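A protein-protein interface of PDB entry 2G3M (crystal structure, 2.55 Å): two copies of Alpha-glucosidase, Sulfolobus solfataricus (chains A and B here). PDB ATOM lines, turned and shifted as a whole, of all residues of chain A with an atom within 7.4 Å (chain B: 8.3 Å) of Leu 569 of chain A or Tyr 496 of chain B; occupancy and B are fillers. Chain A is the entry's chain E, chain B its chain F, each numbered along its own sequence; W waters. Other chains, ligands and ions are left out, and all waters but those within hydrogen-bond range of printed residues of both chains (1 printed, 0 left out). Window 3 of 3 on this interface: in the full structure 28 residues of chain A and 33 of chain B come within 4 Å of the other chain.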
ATOM      1  N   ASP A 542      -0.216  16.879  18.324  1.00  0.00           N
ATOM      2  CA  ASP A 542       1.165  16.464  18.535  1.00  0.00           C
ATOM      3  C   ASP A 542       1.382  14.993  18.169  1.00  0.00           C
ATOM      4  O   ASP A 542       2.427  14.628  17.642  1.00  0.00           O
ATOM      5  CB  ASP A 542       1.548  16.664  20.002  1.00  0.00           C
ATOM      6  CG  ASP A 542       1.887  18.101  20.329  1.00  0.00           C
ATOM      7  OD1 ASP A 542       1.316  19.015  19.692  1.00  0.00           O
ATOM      8  OD2 ASP A 542       2.721  18.313  21.238  1.00  0.00           O
ATOM      9  N   ASP A 548       8.200   7.233  16.083  1.00  0.00           N
ATOM     10  CA  ASP A 548       9.152   6.256  16.597  1.00  0.00           C
ATOM     11  C   ASP A 548       8.598   5.628  17.870  1.00  0.00           C
ATOM     12  O   ASP A 548       9.332   5.088  18.687  1.00  0.00           O
ATOM     13  CB  ASP A 548      10.521   6.899  16.861  1.00  0.00           C
ATOM     14  CG  ASP A 548      10.426   8.196  17.646  1.00  0.00           C
ATOM     15  OD1 ASP A 548       9.395   8.421  18.325  1.00  0.00           O
ATOM     16  OD2 ASP A 548      11.398   8.986  17.592  1.00  0.00           O
ATOM     17  N   GLU A 549       7.283   5.709  18.024  1.00  0.00           N
ATOM     18  CA  GLU A 549       6.593   5.143  19.181  1.00  0.00           C
ATOM     19  C   GLU A 549       5.300   4.517  18.697  1.00  0.00           C
ATOM     20  O   GLU A 549       4.724   4.967  17.706  1.00  0.00           O
ATOM     21  CB  GLU A 549       6.243   6.236  20.204  1.00  0.00           C
ATOM     22  CG  GLU A 549       7.418   6.820  20.959  1.00  0.00           C
ATOM     23  CD  GLU A 549       7.007   7.970  21.849  1.00  0.00           C
ATOM     24  OE1 GLU A 549       5.950   7.871  22.508  1.00  0.00           O
ATOM     25  OE2 GLU A 549       7.745   8.972  21.902  1.00  0.00           O
ATOM     26  N   ALA A 559       8.331   2.737  23.128  1.00  0.00           N
ATOM     27  CA  ALA A 559       9.157   3.714  22.433  1.00  0.00           C
ATOM     28  C   ALA A 559      10.490   3.027  22.159  1.00  0.00           C
ATOM     29  O   ALA A 559      11.466   3.216  22.883  1.00  0.00           O
ATOM     30  CB  ALA A 559       9.358   4.947  23.309  1.00  0.00           C
ATOM     31  N   PRO A 560      10.547   2.206  21.104  1.00  0.00           N
ATOM     32  CA  PRO A 560      11.796   1.507  20.790  1.00  0.00           C
ATOM     33  C   PRO A 560      12.960   2.443  20.508  1.00  0.00           C
ATOM     34  O   PRO A 560      12.790   3.526  19.940  1.00  0.00           O
ATOM     35  CB  PRO A 560      11.419   0.655  19.583  1.00  0.00           C
ATOM     36  CG  PRO A 560      10.367   1.488  18.907  1.00  0.00           C
ATOM     37  CD  PRO A 560       9.533   1.973  20.060  1.00  0.00           C
ATOM     38  N   GLU A 565      22.286   5.818  20.291  1.00  0.00           N
ATOM     39  CA  GLU A 565      22.205   6.280  21.674  1.00  0.00           C
ATOM     40  C   GLU A 565      21.767   5.169  22.638  1.00  0.00           C
ATOM     41  O   GLU A 565      21.192   4.161  22.228  1.00  0.00           O
ATOM     42  CB  GLU A 565      21.234   7.455  21.764  1.00  0.00           C
ATOM     43  CG  GLU A 565      21.646   8.666  20.937  1.00  0.00           C
ATOM     44  CD  GLU A 565      20.602   9.779  20.965  1.00  0.00           C
ATOM     45  OE1 GLU A 565      20.203  10.203  22.076  1.00  0.00           O
ATOM     46  OE2 GLU A 565      20.181  10.231  19.876  1.00  0.00           O
ATOM     47  N   SER A 567      20.003   6.032  25.389  1.00  0.00           N
ATOM     48  CA  SER A 567      18.770   6.575  25.922  1.00  0.00           C
ATOM     49  C   SER A 567      18.116   7.450  24.856  1.00  0.00           C
ATOM     50  O   SER A 567      18.794   7.995  23.985  1.00  0.00           O
ATOM     51  CB  SER A 567      19.082   7.405  27.169  1.00  0.00           C
ATOM     52  OG  SER A 567      17.909   7.974  27.720  1.00  0.00           O
ATOM     53  N   ARG A 568      16.799   7.577  24.914  1.00  0.00           N
ATOM     54  CA  ARG A 568      16.102   8.402  23.946  1.00  0.00           C
ATOM     55  C   ARG A 568      15.076   9.261  24.658  1.00  0.00           C
ATOM     56  O   ARG A 568      14.849   9.117  25.855  1.00  0.00           O
ATOM     57  CB  ARG A 568      15.386   7.530  22.909  1.00  0.00           C
ATOM     58  CG  ARG A 568      14.374   6.564  23.515  1.00  0.00           C
ATOM     59  CD  ARG A 568      13.384   6.072  22.483  1.00  0.00           C
ATOM     60  NE  ARG A 568      12.470   7.131  22.065  1.00  0.00           N
ATOM     61  CZ  ARG A 568      11.613   7.016  21.055  1.00  0.00           C
ATOM     62  NH1 ARG A 568      11.553   5.890  20.363  1.00  0.00           N
ATOM     63  NH2 ARG A 568      10.827   8.030  20.727  1.00  0.00           N
ATOM     64  N   LEU A 569      14.465  10.168  23.916  1.00  0.00           N
ATOM     65  CA  LEU A 569      13.430  11.003  24.474  1.00  0.00           C
ATOM     66  C   LEU A 569      12.103  10.292  24.183  1.00  0.00           C
ATOM     67  O   LEU A 569      11.898   9.774  23.081  1.00  0.00           O
ATOM     68  CB  LEU A 569      13.456  12.396  23.832  1.00  0.00           C
ATOM     69  CG  LEU A 569      14.684  13.260  24.169  1.00  0.00           C
ATOM     70  CD1 LEU A 569      14.577  14.606  23.475  1.00  0.00           C
ATOM     71  CD2 LEU A 569      14.788  13.452  25.689  1.00  0.00           C
ATOM     72  N   VAL A 570      11.220  10.243  25.180  1.00  0.00           N
ATOM     73  CA  VAL A 570       9.928   9.601  25.000  1.00  0.00           C
ATOM     74  C   VAL A 570       8.807  10.609  25.180  1.00  0.00           C
ATOM     75  O   VAL A 570       8.746  11.309  26.186  1.00  0.00           O
ATOM     76  CB  VAL A 570       9.719   8.457  26.007  1.00  0.00           C
ATOM     77  CG1 VAL A 570       8.349   7.826  25.795  1.00  0.00           C
ATOM     78  CG2 VAL A 570      10.828   7.419  25.854  1.00  0.00           C
ATOM     79  N   THR A 571       7.930  10.692  24.190  1.00  0.00           N
ATOM     80  CA  THR A 571       6.795  11.596  24.260  1.00  0.00           C
ATOM     81  C   THR A 571       5.618  10.797  24.806  1.00  0.00           C
ATOM     82  O   THR A 571       5.260   9.749  24.272  1.00  0.00           O
ATOM     83  CB  THR A 571       6.433  12.146  22.878  1.00  0.00           C
ATOM     84  OG1 THR A 571       7.548  12.877  22.351  1.00  0.00           O
ATOM     85  CG2 THR A 571       5.225  13.068  22.969  1.00  0.00           C
ATOM     86  N   LEU A 572       5.037  11.288  25.891  1.00  0.00           N
ATOM     87  CA  LEU A 572       3.916  10.614  26.519  1.00  0.00           C
ATOM     88  C   LEU A 572       2.628  11.377  26.272  1.00  0.00           C
ATOM     89  O   LEU A 572       2.579  12.598  26.433  1.00  0.00           O
ATOM     90  CB  LEU A 572       4.155  10.481  28.025  1.00  0.00           C
ATOM     91  CG  LEU A 572       5.329   9.606  28.481  1.00  0.00           C
ATOM     92  CD1 LEU A 572       5.533   9.766  29.978  1.00  0.00           C
ATOM     93  CD2 LEU A 572       5.062   8.149  28.126  1.00  0.00           C
ATOM     94  N   LYS A 589       1.473  13.976  28.585  1.00  0.00           N
ATOM     95  CA  LYS A 589       1.643  15.195  27.828  1.00  0.00           C
ATOM     96  C   LYS A 589       2.932  15.814  28.335  1.00  0.00           C
ATOM     97  O   LYS A 589       2.955  16.918  28.874  1.00  0.00           O
ATOM     98  CB  LYS A 589       0.449  16.123  28.031  1.00  0.00           C
ATOM     99  CG  LYS A 589       0.291  17.134  26.918  1.00  0.00           C
ATOM    100  CD  LYS A 589       0.323  16.451  25.564  1.00  0.00           C
ATOM    101  CE  LYS A 589       0.465  17.467  24.444  1.00  0.00           C
ATOM    102  NZ  LYS A 589       0.861  16.803  23.175  1.00  0.00           N
ATOM    103  N   SER A 590       4.007  15.051  28.173  1.00  0.00           N
ATOM    104  CA  SER A 590       5.333  15.473  28.583  1.00  0.00           C
ATOM    105  C   SER A 590       6.370  14.641  27.835  1.00  0.00           C
ATOM    106  O   SER A 590       6.043  13.658  27.183  1.00  0.00           O
ATOM    107  CB  SER A 590       5.517  15.279  30.089  1.00  0.00           C
ATOM    108  OG  SER A 590       5.595  13.902  30.412  1.00  0.00           O
ATOM    109  N   VAL A 591       7.626  15.051  27.936  1.00  0.00           N
ATOM    110  CA  VAL A 591       8.720  14.351  27.290  1.00  0.00           C
ATOM    111  C   VAL A 591       9.704  13.922  28.376  1.00  0.00           C
ATOM    112  O   VAL A 591      10.197  14.748  29.148  1.00  0.00           O
ATOM    113  CB  VAL A 591       9.437  15.260  26.263  1.00  0.00           C
ATOM    114  CG1 VAL A 591      10.652  14.550  25.686  1.00  0.00           C
ATOM    115  CG2 VAL A 591       8.479  15.628  25.152  1.00  0.00           C
ATOM    116  N   VAL A 592       9.975  12.625  28.443  1.00  0.00           N
ATOM    117  CA  VAL A 592      10.889  12.105  29.441  1.00  0.00           C
ATOM    118  C   VAL A 592      11.990  11.294  28.784  1.00  0.00           C
ATOM    119  O   VAL A 592      11.908  10.946  27.612  1.00  0.00           O
ATOM    120  CB  VAL A 592      10.145  11.221  30.466  1.00  0.00           C
ATOM    121  CG1 VAL A 592       8.970  11.991  31.044  1.00  0.00           C
ATOM    122  CG2 VAL A 592       9.669   9.925  29.805  1.00  0.00           C
ATOM    123  N   LYS A 593      13.030  11.003  29.550  1.00  0.00           N
ATOM    124  CA  LYS A 593      14.147  10.224  29.053  1.00  0.00           C
ATOM    125  C   LYS A 593      13.930   8.751  29.399  1.00  0.00           C
ATOM    126  O   LYS A 593      13.508   8.415  30.516  1.00  0.00           O
ATOM    127  CB  LYS A 593      15.442  10.749  29.680  1.00  0.00           C
ATOM    128  CG  LYS A 593      16.686   9.951  29.359  1.00  0.00           C
ATOM    129  CD  LYS A 593      17.917  10.541  30.059  1.00  0.00           C
ATOM    130  CE  LYS A 593      19.139   9.633  29.909  1.00  0.00           C
ATOM    131  NZ  LYS A 593      20.387  10.236  30.460  1.00  0.00           N
ATOM    132  N   SER A 594      14.205   7.881  28.423  1.00  0.00           N
ATOM    133  CA  SER A 594      14.063   6.442  28.612  1.00  0.00           C
ATOM    134  C   SER A 594      15.056   6.006  29.683  1.00  0.00           C
ATOM    135  O   SER A 594      16.078   6.658  29.898  1.00  0.00           O
ATOM    136  CB  SER A 594      14.312   5.679  27.298  1.00  0.00           C
ATOM    137  OG  SER A 594      15.661   5.762  26.862  1.00  0.00           O
ATOM    138  N   TYR A 601       5.786   1.438  28.723  1.00  0.00           N
ATOM    139  CA  TYR A 601       4.936   2.142  29.676  1.00  0.00           C
ATOM    140  C   TYR A 601       3.498   1.640  29.617  1.00  0.00           C
ATOM    141  O   TYR A 601       2.988   1.316  28.547  1.00  0.00           O
ATOM    142  CB  TYR A 601       4.947   3.642  29.390  1.00  0.00           C
ATOM    143  CG  TYR A 601       6.325   4.258  29.344  1.00  0.00           C
ATOM    144  CD1 TYR A 601       7.137   4.117  28.220  1.00  0.00           C
ATOM    145  CD2 TYR A 601       6.830   4.963  30.438  1.00  0.00           C
ATOM    146  CE1 TYR A 601       8.421   4.660  28.186  1.00  0.00           C
ATOM    147  CE2 TYR A 601       8.115   5.512  30.421  1.00  0.00           C
ATOM    148  CZ  TYR A 601       8.906   5.356  29.295  1.00  0.00           C
ATOM    149  OH  TYR A 601      10.187   5.880  29.278  1.00  0.00           O
ATOM    150  N   MET B 461      12.562  16.084  13.087  1.00  0.00           N
ATOM    151  CA  MET B 461      12.307  17.318  13.812  1.00  0.00           C
ATOM    152  C   MET B 461      13.477  17.923  14.579  1.00  0.00           C
ATOM    153  O   MET B 461      13.585  19.142  14.665  1.00  0.00           O
ATOM    154  CB  MET B 461      11.111  17.119  14.741  1.00  0.00           C
ATOM    155  CG  MET B 461       9.862  16.747  13.966  1.00  0.00           C
ATOM    156  SD  MET B 461       8.408  16.486  14.980  1.00  0.00           S
ATOM    157  CE  MET B 461       8.769  14.904  15.685  1.00  0.00           C
ATOM    158  N   ASP B 462      14.353  17.094  15.130  1.00  0.00           N
ATOM    159  CA  ASP B 462      15.488  17.636  15.860  1.00  0.00           C
ATOM    160  C   ASP B 462      16.472  18.301  14.895  1.00  0.00           C
ATOM    161  O   ASP B 462      17.162  19.254  15.263  1.00  0.00           O
ATOM    162  CB  ASP B 462      16.166  16.546  16.704  1.00  0.00           C
ATOM    163  CG  ASP B 462      16.603  15.349  15.884  1.00  0.00           C
ATOM    164  OD1 ASP B 462      15.971  15.075  14.837  1.00  0.00           O
ATOM    165  OD2 ASP B 462      17.571  14.667  16.301  1.00  0.00           O
ATOM    166  N   VAL B 465      15.163  21.778  14.090  1.00  0.00           N
ATOM    167  CA  VAL B 465      15.487  22.707  15.163  1.00  0.00           C
ATOM    168  C   VAL B 465      16.929  23.180  15.012  1.00  0.00           C
ATOM    169  O   VAL B 465      17.226  24.365  15.185  1.00  0.00           O
ATOM    170  CB  VAL B 465      15.291  22.052  16.546  1.00  0.00           C
ATOM    171  CG1 VAL B 465      15.820  22.971  17.651  1.00  0.00           C
ATOM    172  CG2 VAL B 465      13.804  21.775  16.768  1.00  0.00           C
ATOM    173  N   LYS B 466      17.823  22.261  14.668  1.00  0.00           N
ATOM    174  CA  LYS B 466      19.220  22.622  14.495  1.00  0.00           C
ATOM    175  C   LYS B 466      19.423  23.594  13.333  1.00  0.00           C
ATOM    176  O   LYS B 466      20.390  24.356  13.322  1.00  0.00           O
ATOM    177  CB  LYS B 466      20.068  21.369  14.316  1.00  0.00           C
ATOM    178  CG  LYS B 466      20.230  20.580  15.617  1.00  0.00           C
ATOM    179  CD  LYS B 466      21.015  21.379  16.644  1.00  0.00           C
ATOM    180  CE  LYS B 466      21.150  20.638  17.974  1.00  0.00           C
ATOM    181  NZ  LYS B 466      19.898  20.722  18.785  1.00  0.00           N
ATOM    182  N   LEU B 493       4.557  21.553  14.665  1.00  0.00           N
ATOM    183  CA  LEU B 493       5.460  20.716  15.442  1.00  0.00           C
ATOM    184  C   LEU B 493       4.883  20.368  16.824  1.00  0.00           C
ATOM    185  O   LEU B 493       4.089  21.119  17.385  1.00  0.00           O
ATOM    186  CB  LEU B 493       6.795  21.436  15.642  1.00  0.00           C
ATOM    187  CG  LEU B 493       7.767  21.616  14.476  1.00  0.00           C
ATOM    188  CD1 LEU B 493       8.885  22.565  14.895  1.00  0.00           C
ATOM    189  CD2 LEU B 493       8.334  20.263  14.079  1.00  0.00           C
ATOM    190  N   PRO B 494       5.272  19.211  17.383  1.00  0.00           N
ATOM    191  CA  PRO B 494       4.777  18.818  18.706  1.00  0.00           C
ATOM    192  C   PRO B 494       5.276  19.894  19.674  1.00  0.00           C
ATOM    193  O   PRO B 494       6.326  20.490  19.437  1.00  0.00           O
ATOM    194  CB  PRO B 494       5.463  17.477  18.948  1.00  0.00           C
ATOM    195  CG  PRO B 494       5.664  16.939  17.567  1.00  0.00           C
ATOM    196  CD  PRO B 494       6.107  18.150  16.795  1.00  0.00           C
ATOM    197  N   ASP B 495       4.540  20.138  20.756  1.00  0.00           N
ATOM    198  CA  ASP B 495       4.919  21.170  21.719  1.00  0.00           C
ATOM    199  C   ASP B 495       6.408  21.215  22.065  1.00  0.00           C
ATOM    200  O   ASP B 495       7.010  22.291  22.104  1.00  0.00           O
ATOM    201  CB  ASP B 495       4.093  21.026  22.999  1.00  0.00           C
ATOM    202  CG  ASP B 495       2.598  21.200  22.751  1.00  0.00           C
ATOM    203  OD1 ASP B 495       2.223  22.116  21.975  1.00  0.00           O
ATOM    204  OD2 ASP B 495       1.796  20.426  23.337  1.00  0.00           O
ATOM    205  N   TYR B 496       7.002  20.052  22.310  1.00  0.00           N
ATOM    206  CA  TYR B 496       8.419  19.974  22.653  1.00  0.00           C
ATOM    207  C   TYR B 496       9.324  20.709  21.656  1.00  0.00           C
ATOM    208  O   TYR B 496      10.162  21.525  22.051  1.00  0.00           O
ATOM    209  CB  TYR B 496       8.851  18.515  22.741  1.00  0.00           C
ATOM    210  CG  TYR B 496      10.316  18.334  23.056  1.00  0.00           C
ATOM    211  CD1 TYR B 496      10.802  18.509  24.352  1.00  0.00           C
ATOM    212  CD2 TYR B 496      11.223  17.990  22.053  1.00  0.00           C
ATOM    213  CE1 TYR B 496      12.160  18.344  24.643  1.00  0.00           C
ATOM    214  CE2 TYR B 496      12.579  17.825  22.329  1.00  0.00           C
ATOM    215  CZ  TYR B 496      13.038  18.004  23.624  1.00  0.00           C
ATOM    216  OH  TYR B 496      14.380  17.846  23.879  1.00  0.00           O
ATOM    217  N   TYR B 497       9.158  20.421  20.367  1.00  0.00           N
ATOM    218  CA  TYR B 497       9.977  21.056  19.333  1.00  0.00           C
ATOM    219  C   TYR B 497       9.502  22.463  18.991  1.00  0.00           C
ATOM    220  O   TYR B 497      10.305  23.337  18.649  1.00  0.00           O
ATOM    221  CB  TYR B 497       9.987  20.192  18.070  1.00  0.00           C
ATOM    222  CG  TYR B 497      10.683  18.870  18.264  1.00  0.00           C
ATOM    223  CD1 TYR B 497      12.072  18.804  18.372  1.00  0.00           C
ATOM    224  CD2 TYR B 497       9.954  17.688  18.385  1.00  0.00           C
ATOM    225  CE1 TYR B 497      12.719  17.592  18.597  1.00  0.00           C
ATOM    226  CE2 TYR B 497      10.593  16.468  18.613  1.00  0.00           C
ATOM    227  CZ  TYR B 497      11.973  16.428  18.718  1.00  0.00           C
ATOM    228  OH  TYR B 497      12.613  15.226  18.950  1.00  0.00           O
ATOM    229  N   LYS B 498       8.194  22.682  19.076  1.00  0.00           N
ATOM    230  CA  LYS B 498       7.641  23.993  18.779  1.00  0.00           C
ATOM    231  C   LYS B 498       8.223  25.049  19.710  1.00  0.00           C
ATOM    232  O   LYS B 498       8.580  26.142  19.273  1.00  0.00           O
ATOM    233  CB  LYS B 498       6.116  23.971  18.892  1.00  0.00           C
ATOM    234  CG  LYS B 498       5.476  25.348  18.771  1.00  0.00           C
ATOM    235  CD  LYS B 498       4.005  25.248  18.427  1.00  0.00           C
ATOM    236  CE  LYS B 498       3.242  24.425  19.450  1.00  0.00           C
ATOM    237  NZ  LYS B 498       1.913  23.989  18.921  1.00  0.00           N
ATOM    238  N   GLU B 499       8.319  24.720  20.994  1.00  0.00           N
ATOM    239  CA  GLU B 499       8.879  25.646  21.969  1.00  0.00           C
ATOM    240  C   GLU B 499      10.346  25.951  21.690  1.00  0.00           C
ATOM    241  O   GLU B 499      10.794  27.087  21.860  1.00  0.00           O
ATOM    242  CB  GLU B 499       8.740  25.089  23.392  1.00  0.00           C
ATOM    243  CG  GLU B 499       7.530  25.623  24.125  1.00  0.00           C
ATOM    244  CD  GLU B 499       7.422  27.138  24.020  1.00  0.00           C
ATOM    245  OE1 GLU B 499       8.379  27.836  24.433  1.00  0.00           O
ATOM    246  OE2 GLU B 499       6.379  27.627  23.517  1.00  0.00           O
ATOM    247  N   LYS B 500      11.103  24.943  21.276  1.00  0.00           N
ATOM    248  CA  LYS B 500      12.507  25.171  20.986  1.00  0.00           C
ATOM    249  C   LYS B 500      12.685  26.170  19.850  1.00  0.00           C
ATOM    250  O   LYS B 500      13.533  27.059  19.930  1.00  0.00           O
ATOM    251  CB  LYS B 500      13.203  23.861  20.641  1.00  0.00           C
ATOM    252  CG  LYS B 500      13.474  22.983  21.840  1.00  0.00           C
ATOM    253  CD  LYS B 500      14.230  21.734  21.425  1.00  0.00           C
ATOM    254  CE  LYS B 500      14.579  20.876  22.624  1.00  0.00           C
ATOM    255  NZ  LYS B 500      15.421  21.631  23.588  1.00  0.00           N
ATOM    256  N   VAL B 501      11.884  26.033  18.796  1.00  0.00           N
ATOM    257  CA  VAL B 501      11.976  26.942  17.664  1.00  0.00           C
ATOM    258  C   VAL B 501      11.557  28.326  18.129  1.00  0.00           C
ATOM    259  O   VAL B 501      12.214  29.321  17.822  1.00  0.00           O
ATOM    260  CB  VAL B 501      11.063  26.488  16.492  1.00  0.00           C
ATOM    261  CG1 VAL B 501      11.094  27.521  15.355  1.00  0.00           C
ATOM    262  CG2 VAL B 501      11.519  25.129  15.973  1.00  0.00           C
ATOM    263  N   LYS B 502      10.466  28.378  18.884  1.00  0.00           N
ATOM    264  CA  LYS B 502       9.942  29.638  19.406  1.00  0.00           C
ATOM    265  C   LYS B 502      11.016  30.420  20.176  1.00  0.00           C
ATOM    266  O   LYS B 502      11.206  31.614  19.948  1.00  0.00           O
ATOM    267  CB  LYS B 502       8.738  29.347  20.307  1.00  0.00           C
ATOM    268  CG  LYS B 502       7.922  30.556  20.735  1.00  0.00           C
ATOM    269  CD  LYS B 502       6.631  30.094  21.411  1.00  0.00           C
ATOM    270  CE  LYS B 502       5.793  31.258  21.930  1.00  0.00           C
ATOM    271  NZ  LYS B 502       6.469  32.017  23.029  1.00  0.00           N
ATOM    272  N   GLU B 503      11.729  29.741  21.068  1.00  0.00           N
ATOM    273  CA  GLU B 503      12.769  30.397  21.857  1.00  0.00           C
ATOM    274  C   GLU B 503      13.919  30.885  20.989  1.00  0.00           C
ATOM    275  O   GLU B 503      14.462  31.965  21.223  1.00  0.00           O
ATOM    276  CB  GLU B 503      13.313  29.448  22.924  1.00  0.00           C
ATOM    277  CG  GLU B 503      12.238  28.874  23.814  1.00  0.00           C
ATOM    278  CD  GLU B 503      12.799  28.057  24.960  1.00  0.00           C
ATOM    279  OE1 GLU B 503      13.744  27.265  24.729  1.00  0.00           O
ATOM    280  OE2 GLU B 503      12.280  28.199  26.090  1.00  0.00           O
ATOM    281  N   GLU B 566      24.854  16.786  23.053  1.00  0.00           N
ATOM    282  CA  GLU B 566      24.262  17.830  23.889  1.00  0.00           C
ATOM    283  C   GLU B 566      25.226  19.011  23.872  1.00  0.00           C
ATOM    284  O   GLU B 566      24.821  20.173  23.941  1.00  0.00           O
ATOM    285  CB  GLU B 566      24.103  17.355  25.339  1.00  0.00           C
ATOM    286  CG  GLU B 566      23.206  16.144  25.536  1.00  0.00           C
ATOM    287  CD  GLU B 566      23.128  15.713  26.995  1.00  0.00           C
ATOM    288  OE1 GLU B 566      24.194  15.474  27.612  1.00  0.00           O
ATOM    289  OE2 GLU B 566      21.999  15.608  27.523  1.00  0.00           O
ATOM    290  N   GLU B 597      22.794  25.102  24.884  1.00  0.00           N
ATOM    291  CA  GLU B 597      22.285  24.563  23.627  1.00  0.00           C
ATOM    292  C   GLU B 597      22.751  25.435  22.455  1.00  0.00           C
ATOM    293  O   GLU B 597      22.916  24.952  21.335  1.00  0.00           O
ATOM    294  CB  GLU B 597      20.764  24.544  23.685  1.00  0.00           C
ATOM    295  CG  GLU B 597      20.108  23.301  23.149  1.00  0.00           C
ATOM    296  CD  GLU B 597      18.612  23.308  23.422  1.00  0.00           C
ATOM    297  OE1 GLU B 597      17.932  24.286  23.008  1.00  0.00           O
ATOM    298  OE2 GLU B 597      18.116  22.344  24.053  1.00  0.00           O
HETATM  299  O   HOH W   1       5.814  17.296  22.464  1.00  0.00           O
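OD2 of Asp 542 of chain A lies within hydrogen-bond range of N of Asp 495 of chain B.
The side-chain carboxylate of Asp 495 of chain B is in salt-bridge range of the side-chain amino group of Lys 589 of chain A, at 3.7 Å.
Water W1 bridges N of Tyr 496 of chain B (3.0 Å) and OD2 of Asp 542 of chain A (3.5 Å).
Of the 19 printed residues of chain A, 4 touch a printed residue of chain B.
Along chain A the printed residues that touch a printed residue of chain B span positions 542 to 591.
Of the 17 printed residues of chain B, 3 touch a printed residue of chain A.
Hydrophobic or aromatic side chains of chain B within 4 Å of the printed part of chain A: Pro 494 and Tyr 496.
Along chain B the printed residues that touch a printed residue of chain A span positions 494 to 496.
Among the printed residues, 5 pairs touch across the chains.
Of the printed residues of chain B, Asp 542 of chain A touches Pro 494 and Asp 495.
Of chain B, only Tyr 496 comes within 4 Å of Leu 569 of chain A.
Printed residues of chain B within 4 Å of Val 591 of chain A: Tyr 496 (3.8 Å).
Of the printed residues of chain A, Asp 495 of chain B touches Asp 542 and Lys 589.
Tyr 496 of chain B touches two residues of chain A.
No position is printed for both chains.
Of the 5 pairs that touch across the chains among the printed residues, none has its exchanged pair printed and touching as well.
The side-chain carboxylate of Asp 542 of chain A lies within salt-bridge range of the side-chain amino group of Lys 589 of chain A (3.1 Å).
O of Leu 572 of chain A sits at hydrogen-bond distance from N of Lys 589 of chain A, at 2.8 Å.
The side-chain carboxylate (OD1) of Asp 495 of chain B lies within salt-bridge range of the side-chain amino group (NZ) of Lys 498 of chain B (3.6 Å).
Among the printed residues, merely in contact across the chains: Asp 542 of chain A with Pro 494 of chain B (3.3 Å), Leu 569 of chain A with Tyr 496 of chain B (3.3 Å) and Val 591 of chain A with Tyr 496 of chain B (3.8 Å).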
